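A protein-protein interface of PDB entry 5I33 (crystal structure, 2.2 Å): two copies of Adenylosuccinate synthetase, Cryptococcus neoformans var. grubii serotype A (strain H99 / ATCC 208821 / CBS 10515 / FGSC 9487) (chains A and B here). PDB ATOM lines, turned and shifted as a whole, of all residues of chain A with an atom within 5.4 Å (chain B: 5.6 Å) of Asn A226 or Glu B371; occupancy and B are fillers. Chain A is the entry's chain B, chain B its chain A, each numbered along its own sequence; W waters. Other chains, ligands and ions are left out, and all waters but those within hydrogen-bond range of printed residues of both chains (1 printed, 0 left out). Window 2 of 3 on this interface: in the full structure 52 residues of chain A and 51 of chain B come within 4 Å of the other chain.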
ATOM      1  N   PRO A 221       5.150 -16.086  23.819  1.00  0.00           N
ATOM      2  CA  PRO A 221       3.824 -16.535  23.389  1.00  0.00           C
ATOM      3  C   PRO A 221       3.816 -17.950  22.835  1.00  0.00           C
ATOM      4  O   PRO A 221       2.913 -18.716  23.146  1.00  0.00           O
ATOM      5  CB  PRO A 221       3.457 -15.522  22.307  1.00  0.00           C
ATOM      6  CG  PRO A 221       4.087 -14.263  22.802  1.00  0.00           C
ATOM      7  CD  PRO A 221       5.397 -14.682  23.432  1.00  0.00           C
ATOM      8  N   THR A 222       4.802 -18.301  22.028  1.00  0.00           N
ATOM      9  CA  THR A 222       4.819 -19.630  21.422  1.00  0.00           C
ATOM     10  C   THR A 222       5.079 -20.737  22.431  1.00  0.00           C
ATOM     11  O   THR A 222       4.361 -21.745  22.468  1.00  0.00           O
ATOM     12  CB  THR A 222       5.867 -19.699  20.286  1.00  0.00           C
ATOM     13  OG1 THR A 222       5.402 -18.894  19.202  1.00  0.00           O
ATOM     14  CG2 THR A 222       6.054 -21.125  19.813  1.00  0.00           C
ATOM     15  N   PHE A 223       6.105 -20.547  23.250  1.00  0.00           N
ATOM     16  CA  PHE A 223       6.463 -21.546  24.239  1.00  0.00           C
ATOM     17  C   PHE A 223       5.246 -21.883  25.108  1.00  0.00           C
ATOM     18  O   PHE A 223       4.904 -23.052  25.305  1.00  0.00           O
ATOM     19  CB  PHE A 223       7.621 -21.043  25.099  1.00  0.00           C
ATOM     20  CG  PHE A 223       7.840 -21.843  26.358  1.00  0.00           C
ATOM     21  CD1 PHE A 223       8.522 -23.055  26.321  1.00  0.00           C
ATOM     22  CD2 PHE A 223       7.335 -21.397  27.569  1.00  0.00           C
ATOM     23  CE1 PHE A 223       8.707 -23.790  27.468  1.00  0.00           C
ATOM     24  CE2 PHE A 223       7.523 -22.126  28.735  1.00  0.00           C
ATOM     25  CZ  PHE A 223       8.221 -23.321  28.687  1.00  0.00           C
ATOM     26  N   MET A 224       4.575 -20.840  25.590  1.00  0.00           N
ATOM     27  CA  MET A 224       3.468 -21.006  26.526  1.00  0.00           C
ATOM     28  C   MET A 224       2.263 -21.651  25.834  1.00  0.00           C
ATOM     29  O   MET A 224       1.612 -22.542  26.389  1.00  0.00           O
ATOM     30  CB  MET A 224       3.100 -19.650  27.140  1.00  0.00           C
ATOM     31  CG  MET A 224       2.160 -19.714  28.324  1.00  0.00           C
ATOM     32  SD  MET A 224       2.632 -20.790  29.687  1.00  0.00           S
ATOM     33  CE  MET A 224       4.229 -20.118  30.107  1.00  0.00           C
ATOM     34  N   HIS A 225       1.983 -21.215  24.616  1.00  0.00           N
ATOM     35  CA  HIS A 225       0.898 -21.805  23.848  1.00  0.00           C
ATOM     36  C   HIS A 225       1.133 -23.303  23.608  1.00  0.00           C
ATOM     37  O   HIS A 225       0.208 -24.105  23.727  1.00  0.00           O
ATOM     38  CB  HIS A 225       0.719 -21.082  22.510  1.00  0.00           C
ATOM     39  CG  HIS A 225      -0.440 -21.592  21.713  1.00  0.00           C
ATOM     40  ND1 HIS A 225      -0.291 -22.467  20.658  1.00  0.00           N
ATOM     41  CD2 HIS A 225      -1.768 -21.343  21.813  1.00  0.00           C
ATOM     42  CE1 HIS A 225      -1.479 -22.744  20.150  1.00  0.00           C
ATOM     43  NE2 HIS A 225      -2.392 -22.074  20.832  1.00  0.00           N
ATOM     44  N   ASN A 226       2.364 -23.672  23.254  1.00  0.00           N
ATOM     45  CA  ASN A 226       2.705 -25.080  23.047  1.00  0.00           C
ATOM     46  C   ASN A 226       2.577 -25.883  24.344  1.00  0.00           C
ATOM     47  O   ASN A 226       2.108 -27.032  24.348  1.00  0.00           O
ATOM     48  CB  ASN A 226       4.122 -25.220  22.472  1.00  0.00           C
ATOM     49  CG  ASN A 226       4.212 -24.766  21.004  1.00  0.00           C
ATOM     50  OD1 ASN A 226       3.196 -24.474  20.374  1.00  0.00           O
ATOM     51  ND2 ASN A 226       5.429 -24.697  20.470  1.00  0.00           N
ATOM     52  N   ALA A 227       2.994 -25.262  25.443  1.00  0.00           N
ATOM     53  CA  ALA A 227       2.860 -25.868  26.758  1.00  0.00           C
ATOM     54  C   ALA A 227       1.392 -26.148  27.041  1.00  0.00           C
ATOM     55  O   ALA A 227       1.009 -27.279  27.331  1.00  0.00           O
ATOM     56  CB  ALA A 227       3.437 -24.964  27.816  1.00  0.00           C
ATOM     57  N   LEU A 228       0.562 -25.124  26.902  1.00  0.00           N
ATOM     58  CA  LEU A 228      -0.850 -25.304  27.163  1.00  0.00           C
ATOM     59  C   LEU A 228      -1.459 -26.358  26.233  1.00  0.00           C
ATOM     60  O   LEU A 228      -2.179 -27.238  26.706  1.00  0.00           O
ATOM     61  CB  LEU A 228      -1.579 -23.967  27.042  1.00  0.00           C
ATOM     62  CG  LEU A 228      -1.109 -22.939  28.093  1.00  0.00           C
ATOM     63  CD1 LEU A 228      -1.831 -21.606  27.967  1.00  0.00           C
ATOM     64  CD2 LEU A 228      -1.191 -23.471  29.519  1.00  0.00           C
ATOM     65  N   SER A 229      -1.109 -26.309  24.938  1.00  0.00           N
ATOM     66  CA  SER A 229      -1.649 -27.235  23.932  1.00  0.00           C
ATOM     67  C   SER A 229      -1.333 -28.684  24.216  1.00  0.00           C
ATOM     68  O   SER A 229      -2.191 -29.547  24.062  1.00  0.00           O
ATOM     69  CB  SER A 229      -1.099 -26.915  22.534  1.00  0.00           C
ATOM     70  OG  SER A 229      -1.402 -25.591  22.156  1.00  0.00           O
ATOM     71  N   SER A 230      -0.093 -28.945  24.621  1.00  0.00           N
ATOM     72  CA  SER A 230       0.357 -30.306  24.893  1.00  0.00           C
ATOM     73  C   SER A 230       0.021 -30.729  26.327  1.00  0.00           C
ATOM     74  O   SER A 230       0.485 -31.760  26.805  1.00  0.00           O
ATOM     75  CB  SER A 230       1.857 -30.430  24.623  1.00  0.00           C
ATOM     76  OG  SER A 230       2.572 -29.378  25.245  1.00  0.00           O
ATOM     77  N   GLY A 231      -0.769 -29.908  27.012  1.00  0.00           N
ATOM     78  CA  GLY A 231      -1.332 -30.290  28.291  1.00  0.00           C
ATOM     79  C   GLY A 231      -0.421 -30.176  29.494  1.00  0.00           C
ATOM     80  O   GLY A 231      -0.597 -30.923  30.462  1.00  0.00           O
ATOM     81  N   LYS A 232       0.568 -29.282  29.433  1.00  0.00           N
ATOM     82  CA  LYS A 232       1.454 -29.047  30.577  1.00  0.00           C
ATOM     83  C   LYS A 232       0.704 -28.394  31.756  1.00  0.00           C
ATOM     84  O   LYS A 232      -0.259 -27.648  31.560  1.00  0.00           O
ATOM     85  CB  LYS A 232       2.637 -28.154  30.183  1.00  0.00           C
ATOM     86  CG  LYS A 232       3.544 -28.686  29.085  1.00  0.00           C
ATOM     87  CD  LYS A 232       4.376 -29.874  29.531  1.00  0.00           C
ATOM     88  CE  LYS A 232       5.075 -30.495  28.320  1.00  0.00           C
ATOM     89  NZ  LYS A 232       4.060 -30.974  27.343  1.00  0.00           N
ATOM     90  N   GLU B 369      10.438 -22.296   7.582  1.00  0.00           N
ATOM     91  CA  GLU B 369       9.222 -21.752   8.189  1.00  0.00           C
ATOM     92  C   GLU B 369       9.484 -21.129   9.558  1.00  0.00           C
ATOM     93  O   GLU B 369      10.196 -21.701  10.380  1.00  0.00           O
ATOM     94  CB  GLU B 369       8.146 -22.841   8.309  1.00  0.00           C
ATOM     95  CG  GLU B 369       6.781 -22.368   8.868  1.00  0.00           C
ATOM     96  CD  GLU B 369       6.016 -21.398   7.955  1.00  0.00           C
ATOM     97  OE1 GLU B 369       6.383 -21.262   6.761  1.00  0.00           O
ATOM     98  OE2 GLU B 369       5.043 -20.773   8.436  1.00  0.00           O
ATOM     99  N   VAL B 370       8.908 -19.953   9.788  1.00  0.00           N
ATOM    100  CA  VAL B 370       8.973 -19.265  11.076  1.00  0.00           C
ATOM    101  C   VAL B 370       7.732 -19.567  11.901  1.00  0.00           C
ATOM    102  O   VAL B 370       6.617 -19.329  11.442  1.00  0.00           O
ATOM    103  CB  VAL B 370       9.056 -17.736  10.906  1.00  0.00           C
ATOM    104  CG1 VAL B 370       9.088 -17.042  12.264  1.00  0.00           C
ATOM    105  CG2 VAL B 370      10.258 -17.365  10.097  1.00  0.00           C
ATOM    106  N   GLU B 371       7.906 -20.108  13.100  1.00  0.00           N
ATOM    107  CA  GLU B 371       6.765 -20.289  13.992  1.00  0.00           C
ATOM    108  C   GLU B 371       6.414 -18.974  14.707  1.00  0.00           C
ATOM    109  O   GLU B 371       7.299 -18.198  15.075  1.00  0.00           O
ATOM    110  CB  GLU B 371       7.027 -21.404  15.008  1.00  0.00           C
ATOM    111  CG  GLU B 371       5.734 -21.994  15.579  1.00  0.00           C
ATOM    112  CD  GLU B 371       5.959 -23.035  16.673  1.00  0.00           C
ATOM    113  OE1 GLU B 371       7.125 -23.258  17.078  1.00  0.00           O
ATOM    114  OE2 GLU B 371       4.953 -23.608  17.153  1.00  0.00           O
ATOM    115  N   GLY B 372       5.119 -18.726  14.879  1.00  0.00           N
ATOM    116  CA  GLY B 372       4.643 -17.552  15.585  1.00  0.00           C
ATOM    117  C   GLY B 372       5.033 -16.247  14.916  1.00  0.00           C
ATOM    118  O   GLY B 372       5.252 -16.203  13.701  1.00  0.00           O
ATOM    119  N   PHE B 373       5.142 -15.189  15.714  1.00  0.00           N
ATOM    120  CA  PHE B 373       5.495 -13.865  15.217  1.00  0.00           C
ATOM    121  C   PHE B 373       6.794 -13.345  15.848  1.00  0.00           C
ATOM    122  O   PHE B 373       6.978 -13.438  17.053  1.00  0.00           O
ATOM    123  CB  PHE B 373       4.340 -12.904  15.479  1.00  0.00           C
ATOM    124  CG  PHE B 373       4.405 -11.644  14.683  1.00  0.00           C
ATOM    125  CD1 PHE B 373       5.098 -10.537  15.166  1.00  0.00           C
ATOM    126  CD2 PHE B 373       3.784 -11.559  13.437  1.00  0.00           C
ATOM    127  CE1 PHE B 373       5.165  -9.370  14.430  1.00  0.00           C
ATOM    128  CE2 PHE B 373       3.838 -10.392  12.702  1.00  0.00           C
ATOM    129  CZ  PHE B 373       4.529  -9.294  13.201  1.00  0.00           C
ATOM    130  N   PRO B 374       7.709 -12.802  15.026  1.00  0.00           N
ATOM    131  CA  PRO B 374       9.049 -12.430  15.513  1.00  0.00           C
ATOM    132  C   PRO B 374       9.061 -11.157  16.344  1.00  0.00           C
ATOM    133  O   PRO B 374       8.457 -10.157  15.947  1.00  0.00           O
ATOM    134  CB  PRO B 374       9.865 -12.209  14.213  1.00  0.00           C
ATOM    135  CG  PRO B 374       8.981 -12.676  13.109  1.00  0.00           C
ATOM    136  CD  PRO B 374       7.575 -12.583  13.574  1.00  0.00           C
HETATM  137  O   HOH W   1       5.285 -15.604  18.385  1.00  0.00           O
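O of Asn A226 sits at hydrogen-bond distance from OG of Ser A230 (2.6 Å).
Glu B371 touches Thr A222 (OE1 to CG2, 3.6 Å). Thr A222 touches Gly B372. Glu B371 touches Asn A226 (OE2 to ND2, 3.5 Å).
Asn A226 touches just one residue of chain B: Glu B371 (3.5 Å). Glu B371 touches just these residues of chain A: Thr A222 and Asn A226. Of the printed residues of chain B, Thr A222 touches Glu B371 (3.6 Å) and Gly B372 (3.9 Å). Of the printed residues of chain A, Gly B372 touches Thr A222 (3.9 Å). Leu A228 touches none of the printed residues of chain B. The nearest printed residue of chain A that does not touch Glu B371 is His A225 (6.4 Å). The nearest printed residue of chain A that does not touch Gly B372 is Pro A221 (7.1 Å).
Among the printed residues, 3 pairs touch across the chains.
No position is printed for both chains.
Water W1 lies within hydrogen-bond range of N of Phe B373 (2.7 Å) and OG1 of Thr A222 (3.4 Å).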
